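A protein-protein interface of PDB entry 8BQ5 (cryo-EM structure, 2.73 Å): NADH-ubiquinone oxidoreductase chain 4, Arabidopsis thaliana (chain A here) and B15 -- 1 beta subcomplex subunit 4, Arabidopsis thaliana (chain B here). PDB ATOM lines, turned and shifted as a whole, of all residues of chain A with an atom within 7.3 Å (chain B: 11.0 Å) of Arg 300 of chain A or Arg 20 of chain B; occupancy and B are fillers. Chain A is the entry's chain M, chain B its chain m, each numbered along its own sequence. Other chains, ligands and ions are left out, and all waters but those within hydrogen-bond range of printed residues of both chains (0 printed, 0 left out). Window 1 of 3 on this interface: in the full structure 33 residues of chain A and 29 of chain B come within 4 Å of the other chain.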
ATOM      1  N   ARG A 165      15.445  33.500 -15.544  1.00  0.00           N
ATOM      2  CA  ARG A 165      15.893  32.556 -14.526  1.00  0.00           C
ATOM      3  C   ARG A 165      15.827  33.160 -13.127  1.00  0.00           C
ATOM      4  O   ARG A 165      15.913  32.423 -12.132  1.00  0.00           O
ATOM      5  CB  ARG A 165      17.318  32.097 -14.837  1.00  0.00           C
ATOM      6  CG  ARG A 165      17.440  31.183 -16.050  1.00  0.00           C
ATOM      7  CD  ARG A 165      18.759  30.413 -16.046  1.00  0.00           C
ATOM      8  NE  ARG A 165      18.762  29.272 -15.138  1.00  0.00           N
ATOM      9  CZ  ARG A 165      18.087  28.147 -15.342  1.00  0.00           C
ATOM     10  NH1 ARG A 165      17.333  27.978 -16.416  1.00  0.00           N
ATOM     11  NH2 ARG A 165      18.180  27.166 -14.449  1.00  0.00           N
ATOM     12  N   SER A 295      35.694  23.553  -5.535  1.00  0.00           N
ATOM     13  CA  SER A 295      36.777  24.160  -6.305  1.00  0.00           C
ATOM     14  C   SER A 295      36.944  23.467  -7.649  1.00  0.00           C
ATOM     15  O   SER A 295      37.203  24.119  -8.666  1.00  0.00           O
ATOM     16  CB  SER A 295      38.085  24.118  -5.517  1.00  0.00           C
ATOM     17  OG  SER A 295      37.909  24.615  -4.203  1.00  0.00           O
ATOM     18  N   LEU A 296      36.802  22.140  -7.672  1.00  0.00           N
ATOM     19  CA  LEU A 296      36.861  21.413  -8.934  1.00  0.00           C
ATOM     20  C   LEU A 296      35.654  21.728  -9.807  1.00  0.00           C
ATOM     21  O   LEU A 296      35.763  21.763 -11.038  1.00  0.00           O
ATOM     22  CB  LEU A 296      36.969  19.914  -8.666  1.00  0.00           C
ATOM     23  CG  LEU A 296      38.359  19.506  -8.182  1.00  0.00           C
ATOM     24  CD1 LEU A 296      38.429  18.027  -7.860  1.00  0.00           C
ATOM     25  CD2 LEU A 296      39.394  19.879  -9.229  1.00  0.00           C
ATOM     26  N   THR A 297      34.491  21.950  -9.190  1.00  0.00           N
ATOM     27  CA  THR A 297      33.319  22.375  -9.949  1.00  0.00           C
ATOM     28  C   THR A 297      33.531  23.759 -10.553  1.00  0.00           C
ATOM     29  O   THR A 297      33.134  24.012 -11.696  1.00  0.00           O
ATOM     30  CB  THR A 297      32.080  22.362  -9.053  1.00  0.00           C
ATOM     31  OG1 THR A 297      31.694  21.010  -8.792  1.00  0.00           O
ATOM     32  CG2 THR A 297      30.923  23.079  -9.724  1.00  0.00           C
ATOM     33  N   THR A 298      34.163  24.662  -9.799  1.00  0.00           N
ATOM     34  CA  THR A 298      34.434  26.008 -10.299  1.00  0.00           C
ATOM     35  C   THR A 298      35.272  25.964 -11.570  1.00  0.00           C
ATOM     36  O   THR A 298      35.074  26.765 -12.489  1.00  0.00           O
ATOM     37  CB  THR A 298      35.143  26.832  -9.221  1.00  0.00           C
ATOM     38  OG1 THR A 298      34.527  26.597  -7.949  1.00  0.00           O
ATOM     39  CG2 THR A 298      35.073  28.309  -9.546  1.00  0.00           C
ATOM     40  N   LEU A 299      36.217  25.021 -11.633  1.00  0.00           N
ATOM     41  CA  LEU A 299      37.076  24.872 -12.803  1.00  0.00           C
ATOM     42  C   LEU A 299      36.281  24.683 -14.088  1.00  0.00           C
ATOM     43  O   LEU A 299      36.671  25.200 -15.140  1.00  0.00           O
ATOM     44  CB  LEU A 299      38.013  23.680 -12.603  1.00  0.00           C
ATOM     45  CG  LEU A 299      39.452  23.716 -13.120  1.00  0.00           C
ATOM     46  CD1 LEU A 299      40.061  25.101 -13.032  1.00  0.00           C
ATOM     47  CD2 LEU A 299      40.296  22.709 -12.360  1.00  0.00           C
ATOM     48  N   ARG A 300      35.171  23.948 -14.028  1.00  0.00           N
ATOM     49  CA  ARG A 300      34.433  23.552 -15.220  1.00  0.00           C
ATOM     50  C   ARG A 300      33.226  24.439 -15.503  1.00  0.00           C
ATOM     51  O   ARG A 300      32.450  24.136 -16.415  1.00  0.00           O
ATOM     52  CB  ARG A 300      33.998  22.091 -15.102  1.00  0.00           C
ATOM     53  CG  ARG A 300      35.157  21.101 -15.059  1.00  0.00           C
ATOM     54  CD  ARG A 300      36.094  21.282 -16.247  1.00  0.00           C
ATOM     55  NE  ARG A 300      35.412  21.076 -17.520  1.00  0.00           N
ATOM     56  CZ  ARG A 300      35.153  19.889 -18.051  1.00  0.00           C
ATOM     57  NH1 ARG A 300      35.528  18.768 -17.457  1.00  0.00           N
ATOM     58  NH2 ARG A 300      34.501  19.825 -19.207  1.00  0.00           N
ATOM     59  N   GLN A 301      33.041  25.518 -14.751  1.00  0.00           N
ATOM     60  CA  GLN A 301      31.967  26.462 -15.024  1.00  0.00           C
ATOM     61  C   GLN A 301      32.335  27.338 -16.214  1.00  0.00           C
ATOM     62  O   GLN A 301      33.502  27.692 -16.404  1.00  0.00           O
ATOM     63  CB  GLN A 301      31.681  27.324 -13.795  1.00  0.00           C
ATOM     64  CG  GLN A 301      31.232  26.532 -12.578  1.00  0.00           C
ATOM     65  CD  GLN A 301      29.911  25.825 -12.799  1.00  0.00           C
ATOM     66  OE1 GLN A 301      28.928  26.438 -13.213  1.00  0.00           O
ATOM     67  NE2 GLN A 301      29.882  24.526 -12.526  1.00  0.00           N
ATOM     68  N   ILE A 302      31.332  27.680 -17.020  1.00  0.00           N
ATOM     69  CA  ILE A 302      31.528  28.434 -18.254  1.00  0.00           C
ATOM     70  C   ILE A 302      30.958  29.835 -18.174  1.00  0.00           C
ATOM     71  O   ILE A 302      31.070  30.598 -19.144  1.00  0.00           O
ATOM     72  CB  ILE A 302      30.933  27.686 -19.459  1.00  0.00           C
ATOM     73  CG1 ILE A 302      29.410  27.592 -19.324  1.00  0.00           C
ATOM     74  CG2 ILE A 302      31.544  26.306 -19.570  1.00  0.00           C
ATOM     75  CD1 ILE A 302      28.748  26.799 -20.419  1.00  0.00           C
ATOM     76  N   ASP A 303      30.349  30.198 -17.053  1.00  0.00           N
ATOM     77  CA  ASP A 303      29.732  31.498 -16.858  1.00  0.00           C
ATOM     78  C   ASP A 303      30.613  32.316 -15.924  1.00  0.00           C
ATOM     79  O   ASP A 303      31.050  31.814 -14.884  1.00  0.00           O
ATOM     80  CB  ASP A 303      28.316  31.327 -16.295  1.00  0.00           C
ATOM     81  CG  ASP A 303      27.648  32.643 -15.931  1.00  0.00           C
ATOM     82  OD1 ASP A 303      28.228  33.713 -16.185  1.00  0.00           O
ATOM     83  OD2 ASP A 303      26.527  32.603 -15.385  1.00  0.00           O
ATOM     84  N   LYS A 306      29.032  32.537 -12.565  1.00  0.00           N
ATOM     85  CA  LYS A 306      28.967  31.232 -11.914  1.00  0.00           C
ATOM     86  C   LYS A 306      30.316  30.846 -11.323  1.00  0.00           C
ATOM     87  O   LYS A 306      30.377  30.173 -10.289  1.00  0.00           O
ATOM     88  CB  LYS A 306      28.495  30.166 -12.900  1.00  0.00           C
ATOM     89  CG  LYS A 306      26.990  30.055 -13.009  1.00  0.00           C
ATOM     90  CD  LYS A 306      26.443  29.068 -12.003  1.00  0.00           C
ATOM     91  CE  LYS A 306      24.925  29.091 -11.973  1.00  0.00           C
ATOM     92  NZ  LYS A 306      24.346  29.388 -13.314  1.00  0.00           N
ATOM     93  N   ILE A 307      31.407  31.249 -11.975  1.00  0.00           N
ATOM     94  CA  ILE A 307      32.736  30.957 -11.448  1.00  0.00           C
ATOM     95  C   ILE A 307      32.986  31.738 -10.164  1.00  0.00           C
ATOM     96  O   ILE A 307      33.417  31.176  -9.151  1.00  0.00           O
ATOM     97  CB  ILE A 307      33.809  31.257 -12.510  1.00  0.00           C
ATOM     98  CG1 ILE A 307      33.714  30.249 -13.655  1.00  0.00           C
ATOM     99  CG2 ILE A 307      35.198  31.241 -11.889  1.00  0.00           C
ATOM    100  CD1 ILE A 307      34.158  30.790 -14.986  1.00  0.00           C
ATOM    101  N   TYR A 428      41.584  27.933 -11.280  1.00  0.00           N
ATOM    102  CA  TYR A 428      40.432  28.529 -11.947  1.00  0.00           C
ATOM    103  C   TYR A 428      40.536  30.048 -12.011  1.00  0.00           C
ATOM    104  O   TYR A 428      40.036  30.657 -12.962  1.00  0.00           O
ATOM    105  CB  TYR A 428      39.126  28.088 -11.274  1.00  0.00           C
ATOM    106  CG  TYR A 428      38.923  28.520  -9.838  1.00  0.00           C
ATOM    107  CD1 TYR A 428      38.578  29.827  -9.521  1.00  0.00           C
ATOM    108  CD2 TYR A 428      39.030  27.605  -8.802  1.00  0.00           C
ATOM    109  CE1 TYR A 428      38.381  30.215  -8.216  1.00  0.00           C
ATOM    110  CE2 TYR A 428      38.830  27.982  -7.494  1.00  0.00           C
ATOM    111  CZ  TYR A 428      38.507  29.288  -7.206  1.00  0.00           C
ATOM    112  OH  TYR A 428      38.308  29.666  -5.900  1.00  0.00           O
ATOM    113  N   TRP A 431      42.789  30.741 -14.931  1.00  0.00           N
ATOM    114  CA  TRP A 431      42.097  30.323 -16.147  1.00  0.00           C
ATOM    115  C   TRP A 431      41.010  31.319 -16.526  1.00  0.00           C
ATOM    116  O   TRP A 431      40.846  31.657 -17.703  1.00  0.00           O
ATOM    117  CB  TRP A 431      41.500  28.927 -15.975  1.00  0.00           C
ATOM    118  CG  TRP A 431      41.359  28.208 -17.279  1.00  0.00           C
ATOM    119  CD1 TRP A 431      41.969  28.529 -18.456  1.00  0.00           C
ATOM    120  CD2 TRP A 431      40.527  27.075 -17.555  1.00  0.00           C
ATOM    121  NE1 TRP A 431      41.586  27.656 -19.442  1.00  0.00           N
ATOM    122  CE2 TRP A 431      40.699  26.755 -18.917  1.00  0.00           C
ATOM    123  CE3 TRP A 431      39.659  26.296 -16.785  1.00  0.00           C
ATOM    124  CZ2 TRP A 431      40.038  25.689 -19.523  1.00  0.00           C
ATOM    125  CZ3 TRP A 431      39.003  25.238 -17.389  1.00  0.00           C
ATOM    126  CH2 TRP A 431      39.196  24.944 -18.744  1.00  0.00           C
ATOM    127  N   ARG A 435      41.261  33.602 -20.062  1.00  0.00           N
ATOM    128  CA  ARG A 435      40.264  33.377 -21.102  1.00  0.00           C
ATOM    129  C   ARG A 435      39.465  34.640 -21.401  1.00  0.00           C
ATOM    130  O   ARG A 435      38.921  34.781 -22.500  1.00  0.00           O
ATOM    131  CB  ARG A 435      39.333  32.236 -20.696  1.00  0.00           C
ATOM    132  CG  ARG A 435      39.967  30.860 -20.796  1.00  0.00           C
ATOM    133  CD  ARG A 435      39.020  29.781 -20.308  1.00  0.00           C
ATOM    134  NE  ARG A 435      38.655  29.973 -18.910  1.00  0.00           N
ATOM    135  CZ  ARG A 435      37.974  29.097 -18.186  1.00  0.00           C
ATOM    136  NH1 ARG A 435      37.568  27.946 -18.696  1.00  0.00           N
ATOM    137  NH2 ARG A 435      37.692  29.383 -16.919  1.00  0.00           N
ATOM    138  N   LYS B  11      24.007  30.905 -31.912  1.00  0.00           N
ATOM    139  CA  LYS B  11      22.985  29.937 -31.517  1.00  0.00           C
ATOM    140  C   LYS B  11      23.611  28.682 -30.919  1.00  0.00           C
ATOM    141  O   LYS B  11      23.065  28.097 -29.976  1.00  0.00           O
ATOM    142  CB  LYS B  11      22.108  29.585 -32.721  1.00  0.00           C
ATOM    143  CG  LYS B  11      20.662  29.243 -32.377  1.00  0.00           C
ATOM    144  CD  LYS B  11      20.280  27.847 -32.850  1.00  0.00           C
ATOM    145  CE  LYS B  11      18.830  27.523 -32.523  1.00  0.00           C
ATOM    146  NZ  LYS B  11      18.602  27.409 -31.054  1.00  0.00           N
ATOM    147  N   PHE B  12      24.758  28.255 -31.449  1.00  0.00           N
ATOM    148  CA  PHE B  12      25.393  27.046 -30.936  1.00  0.00           C
ATOM    149  C   PHE B  12      26.091  27.307 -29.607  1.00  0.00           C
ATOM    150  O   PHE B  12      26.106  26.439 -28.727  1.00  0.00           O
ATOM    151  CB  PHE B  12      26.371  26.493 -31.968  1.00  0.00           C
ATOM    152  CG  PHE B  12      25.726  26.151 -33.274  1.00  0.00           C
ATOM    153  CD1 PHE B  12      25.055  24.953 -33.437  1.00  0.00           C
ATOM    154  CD2 PHE B  12      25.782  27.033 -34.338  1.00  0.00           C
ATOM    155  CE1 PHE B  12      24.452  24.641 -34.638  1.00  0.00           C
ATOM    156  CE2 PHE B  12      25.182  26.725 -35.543  1.00  0.00           C
ATOM    157  CZ  PHE B  12      24.517  25.527 -35.692  1.00  0.00           C
ATOM    158  N   ILE B  13      26.675  28.494 -29.441  1.00  0.00           N
ATOM    159  CA  ILE B  13      27.257  28.852 -28.152  1.00  0.00           C
ATOM    160  C   ILE B  13      26.161  29.033 -27.109  1.00  0.00           C
ATOM    161  O   ILE B  13      26.308  28.616 -25.953  1.00  0.00           O
ATOM    162  CB  ILE B  13      28.140  30.107 -28.292  1.00  0.00           C
ATOM    163  CG1 ILE B  13      29.413  29.766 -29.066  1.00  0.00           C
ATOM    164  CG2 ILE B  13      28.499  30.671 -26.931  1.00  0.00           C
ATOM    165  CD1 ILE B  13      30.236  30.965 -29.458  1.00  0.00           C
ATOM    166  N   GLU B  14      25.037  29.635 -27.502  1.00  0.00           N
ATOM    167  CA  GLU B  14      23.940  29.833 -26.558  1.00  0.00           C
ATOM    168  C   GLU B  14      23.218  28.529 -26.243  1.00  0.00           C
ATOM    169  O   GLU B  14      22.778  28.321 -25.107  1.00  0.00           O
ATOM    170  CB  GLU B  14      22.965  30.880 -27.091  1.00  0.00           C
ATOM    171  CG  GLU B  14      23.579  32.256 -27.183  1.00  0.00           C
ATOM    172  CD  GLU B  14      23.732  32.898 -25.817  1.00  0.00           C
ATOM    173  OE1 GLU B  14      22.985  32.509 -24.896  1.00  0.00           O
ATOM    174  OE2 GLU B  14      24.605  33.775 -25.661  1.00  0.00           O
ATOM    175  N   ASP B  15      23.062  27.647 -27.233  1.00  0.00           N
ATOM    176  CA  ASP B  15      22.536  26.316 -26.941  1.00  0.00           C
ATOM    177  C   ASP B  15      23.485  25.549 -26.029  1.00  0.00           C
ATOM    178  O   ASP B  15      23.047  24.866 -25.095  1.00  0.00           O
ATOM    179  CB  ASP B  15      22.293  25.541 -28.237  1.00  0.00           C
ATOM    180  CG  ASP B  15      20.958  25.873 -28.874  1.00  0.00           C
ATOM    181  OD1 ASP B  15      20.348  24.968 -29.481  1.00  0.00           O
ATOM    182  OD2 ASP B  15      20.517  27.037 -28.771  1.00  0.00           O
ATOM    183  N   TRP B  16      24.789  25.653 -26.291  1.00  0.00           N
ATOM    184  CA  TRP B  16      25.794  25.121 -25.375  1.00  0.00           C
ATOM    185  C   TRP B  16      25.614  25.689 -23.974  1.00  0.00           C
ATOM    186  O   TRP B  16      25.693  24.960 -22.979  1.00  0.00           O
ATOM    187  CB  TRP B  16      27.188  25.449 -25.906  1.00  0.00           C
ATOM    188  CG  TRP B  16      28.303  24.784 -25.182  1.00  0.00           C
ATOM    189  CD1 TRP B  16      28.498  23.448 -25.020  1.00  0.00           C
ATOM    190  CD2 TRP B  16      29.375  25.435 -24.495  1.00  0.00           C
ATOM    191  NE1 TRP B  16      29.638  23.223 -24.286  1.00  0.00           N
ATOM    192  CE2 TRP B  16      30.193  24.429 -23.950  1.00  0.00           C
ATOM    193  CE3 TRP B  16      29.724  26.774 -24.292  1.00  0.00           C
ATOM    194  CZ2 TRP B  16      31.339  24.718 -23.215  1.00  0.00           C
ATOM    195  CZ3 TRP B  16      30.861  27.058 -23.565  1.00  0.00           C
ATOM    196  CH2 TRP B  16      31.656  26.035 -23.035  1.00  0.00           C
ATOM    197  N   GLY B  17      25.382  26.999 -23.880  1.00  0.00           N
ATOM    198  CA  GLY B  17      25.240  27.626 -22.576  1.00  0.00           C
ATOM    199  C   GLY B  17      23.987  27.188 -21.845  1.00  0.00           C
ATOM    200  O   GLY B  17      24.010  26.948 -20.636  1.00  0.00           O
ATOM    201  N   SER B  18      22.870  27.082 -22.570  1.00  0.00           N
ATOM    202  CA  SER B  18      21.608  26.725 -21.931  1.00  0.00           C
ATOM    203  C   SER B  18      21.542  25.245 -21.585  1.00  0.00           C
ATOM    204  O   SER B  18      20.829  24.861 -20.651  1.00  0.00           O
ATOM    205  CB  SER B  18      20.436  27.114 -22.829  1.00  0.00           C
ATOM    206  OG  SER B  18      20.309  28.523 -22.906  1.00  0.00           O
ATOM    207  N   ALA B  19      22.267  24.400 -22.322  1.00  0.00           N
ATOM    208  CA  ALA B  19      22.322  22.987 -21.967  1.00  0.00           C
ATOM    209  C   ALA B  19      22.899  22.801 -20.573  1.00  0.00           C
ATOM    210  O   ALA B  19      22.387  22.003 -19.780  1.00  0.00           O
ATOM    211  CB  ALA B  19      23.147  22.215 -22.997  1.00  0.00           C
ATOM    212  N   ARG B  20      23.957  23.549 -20.252  1.00  0.00           N
ATOM    213  CA  ARG B  20      24.608  23.419 -18.953  1.00  0.00           C
ATOM    214  C   ARG B  20      23.667  23.786 -17.811  1.00  0.00           C
ATOM    215  O   ARG B  20      23.663  23.127 -16.765  1.00  0.00           O
ATOM    216  CB  ARG B  20      25.864  24.290 -18.919  1.00  0.00           C
ATOM    217  CG  ARG B  20      26.619  24.213 -17.613  1.00  0.00           C
ATOM    218  CD  ARG B  20      27.447  22.943 -17.523  1.00  0.00           C
ATOM    219  NE  ARG B  20      28.162  22.627 -18.755  1.00  0.00           N
ATOM    220  CZ  ARG B  20      29.421  22.968 -18.988  1.00  0.00           C
ATOM    221  NH1 ARG B  20      30.128  23.649 -18.103  1.00  0.00           N
ATOM    222  NH2 ARG B  20      29.990  22.609 -20.137  1.00  0.00           N
ATOM    223  N   GLU B  21      22.865  24.838 -17.985  1.00  0.00           N
ATOM    224  CA  GLU B  21      21.997  25.318 -16.916  1.00  0.00           C
ATOM    225  C   GLU B  21      20.849  24.370 -16.598  1.00  0.00           C
ATOM    226  O   GLU B  21      20.219  24.526 -15.547  1.00  0.00           O
ATOM    227  CB  GLU B  21      21.421  26.688 -17.274  1.00  0.00           C
ATOM    228  CG  GLU B  21      22.333  27.537 -18.120  1.00  0.00           C
ATOM    229  CD  GLU B  21      22.067  29.013 -17.954  1.00  0.00           C
ATOM    230  OE1 GLU B  21      21.646  29.656 -18.939  1.00  0.00           O
ATOM    231  OE2 GLU B  21      22.279  29.532 -16.839  1.00  0.00           O
ATOM    232  N   ASN B  22      20.559  23.408 -17.468  1.00  0.00           N
ATOM    233  CA  ASN B  22      19.420  22.515 -17.309  1.00  0.00           C
ATOM    234  C   ASN B  22      19.881  21.066 -17.237  1.00  0.00           C
ATOM    235  O   ASN B  22      19.293  20.170 -17.847  1.00  0.00           O
ATOM    236  CB  ASN B  22      18.419  22.720 -18.444  1.00  0.00           C
ATOM    237  CG  ASN B  22      17.725  24.066 -18.364  1.00  0.00           C
ATOM    238  OD1 ASN B  22      18.044  24.989 -19.112  1.00  0.00           O
ATOM    239  ND2 ASN B  22      16.768  24.184 -17.451  1.00  0.00           N
ATOM    240  N   LEU B  23      20.949  20.817 -16.473  1.00  0.00           N
ATOM    241  CA  LEU B  23      21.523  19.478 -16.404  1.00  0.00           C
ATOM    242  C   LEU B  23      20.693  18.539 -15.538  1.00  0.00           C
ATOM    243  O   LEU B  23      20.698  17.325 -15.767  1.00  0.00           O
ATOM    244  CB  LEU B  23      22.953  19.547 -15.875  1.00  0.00           C
ATOM    245  CG  LEU B  23      23.967  18.663 -16.598  1.00  0.00           C
ATOM    246  CD1 LEU B  23      23.878  18.865 -18.102  1.00  0.00           C
ATOM    247  CD2 LEU B  23      25.371  18.939 -16.094  1.00  0.00           C
ATOM    248  N   GLU B  24      19.986  19.071 -14.538  1.00  0.00           N
ATOM    249  CA  GLU B  24      19.190  18.218 -13.664  1.00  0.00           C
ATOM    250  C   GLU B  24      18.015  17.578 -14.393  1.00  0.00           C
ATOM    251  O   GLU B  24      17.448  16.601 -13.891  1.00  0.00           O
ATOM    252  CB  GLU B  24      18.685  19.016 -12.460  1.00  0.00           C
ATOM    253  CG  GLU B  24      17.706  20.122 -12.811  1.00  0.00           C
ATOM    254  CD  GLU B  24      18.390  21.400 -13.247  1.00  0.00           C
ATOM    255  OE1 GLU B  24      19.138  21.369 -14.245  1.00  0.00           O
ATOM    256  OE2 GLU B  24      18.169  22.442 -12.596  1.00  0.00           O
ATOM    257  N   HIS B  25      17.635  18.099 -15.561  1.00  0.00           N
ATOM    258  CA  HIS B  25      16.586  17.458 -16.344  1.00  0.00           C
ATOM    259  C   HIS B  25      17.053  16.166 -17.001  1.00  0.00           C
ATOM    260  O   HIS B  25      16.210  15.392 -17.466  1.00  0.00           O
ATOM    261  CB  HIS B  25      16.058  18.406 -17.423  1.00  0.00           C
ATOM    262  CG  HIS B  25      15.497  19.687 -16.889  1.00  0.00           C
ATOM    263  ND1 HIS B  25      15.404  19.957 -15.541  1.00  0.00           N
ATOM    264  CD2 HIS B  25      15.004  20.775 -17.525  1.00  0.00           C
ATOM    265  CE1 HIS B  25      14.877  21.156 -15.369  1.00  0.00           C
ATOM    266  NE2 HIS B  25      14.625  21.673 -16.558  1.00  0.00           N
ATOM    267  N   ASN B  26      18.362  15.988 -17.154  1.00  0.00           N
ATOM    268  CA  ASN B  26      18.854  14.796 -17.892  1.00  0.00           C
ATOM    269  C   ASN B  26      19.328  13.726 -16.909  1.00  0.00           C
ATOM    270  O   ASN B  26      19.810  12.687 -17.386  1.00  0.00           O
ATOM    271  CB  ASN B  26      20.005  15.142 -18.837  1.00  0.00           C
ATOM    272  CG  ASN B  26      19.714  16.320 -19.738  1.00  0.00           C
ATOM    273  OD1 ASN B  26      19.800  17.469 -19.310  1.00  0.00           O
ATOM    274  ND2 ASN B  26      19.380  16.045 -20.989  1.00  0.00           N
ATOM    275  N   PHE B  27      19.185  13.952 -15.602  1.00  0.00           N
ATOM    276  CA  PHE B  27      19.758  12.983 -14.627  1.00  0.00           C
ATOM    277  C   PHE B  27      18.930  11.700 -14.597  1.00  0.00           C
ATOM    278  O   PHE B  27      17.748  11.751 -14.209  1.00  0.00           O
ATOM    279  CB  PHE B  27      19.914  13.597 -13.231  1.00  0.00           C
ATOM    280  CG  PHE B  27      20.494  12.674 -12.189  1.00  0.00           C
ATOM    281  CD1 PHE B  27      21.864  12.518 -12.062  1.00  0.00           C
ATOM    282  CD2 PHE B  27      19.671  11.965 -11.328  1.00  0.00           C
ATOM    283  CE1 PHE B  27      22.399  11.672 -11.103  1.00  0.00           C
ATOM    284  CE2 PHE B  27      20.205  11.117 -10.371  1.00  0.00           C
ATOM    285  CZ  PHE B  27      21.568  10.972 -10.260  1.00  0.00           C
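Leu 296 of chain A touches none of the printed residues of chain B. Thr 298 of chain A touches none of the printed residues of chain B. No residue of chain B comes within 4 Å of Leu 299 of chain A. Arg 300 of chain A touches just one residue of chain B: Arg 20. No residue of chain B comes within 4 Å of Gln 301 of chain A. Printed residues of chain B within 4 Å of Ile 302 of chain A: Trp 16 (3.5 Å) and Arg 20 (3.3 Å). Glu 14 of chain B touches none of the printed residues of chain A. Arg 20 of chain B touches just these residues of chain A: Arg 300 and Ile 302. Of the printed residues of chain A, Glu 21 of chain B touches Arg 165. Printed residues of chain A within 4 Å of Asn 22 of chain B: Arg 165. The nearest residue of chain B that does not touch Arg 300 of chain A is Trp 16 of chain B (6.9 Å). The nearest printed residue of chain B that does not touch Ile 302 of chain A is Gly 17 of chain B (4.2 Å).
The backbone carbonyl oxygen of Arg 300 of chain A is in hydrogen-bond range of the guanidinium group of Arg 20 of chain B, 2.9 Å away. The side-chain carboxylate of Glu 21 of chain B lies within salt-bridge range of the guanidinium group of Arg 165 of chain A.
The backbone carbonyl oxygen (O) of Ser 18 of chain B lies close to the side-chain amide oxygen (OD1) of Asn 22 of chain B (3.2 Å). The side-chain amide oxygen (OD1) of Asn 26 of chain B lies close to the backbone carbonyl oxygen (O) of Asn 22 of chain B (3.1 Å). ND2 of Asn 22 of chain B lies within hydrogen-bond range of NE2 of His 25 of chain B (3.4 Å).
NH1 of Arg 165 of chain A touches ND2 of Asn 22 of chain B, 3.97 Å away. Trp 16 of chain B touches Ile 302 of chain A (CH2 to CG2, 3.5 Å). Arg 20 of chain B touches Ile 302 of chain A.
Printed residues of chain B that touch a printed residue of chain A: Trp 16, Arg 20, Glu 21 and Asn 22. Printed residues of chain A that touch a printed residue of chain B: Arg 165, Arg 300 and Ile 302. Hydrophobic or aromatic side chains of chain A that line the printed part of chain B: Ile 302. Among the printed residues, 5 pairs touch across the chains.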
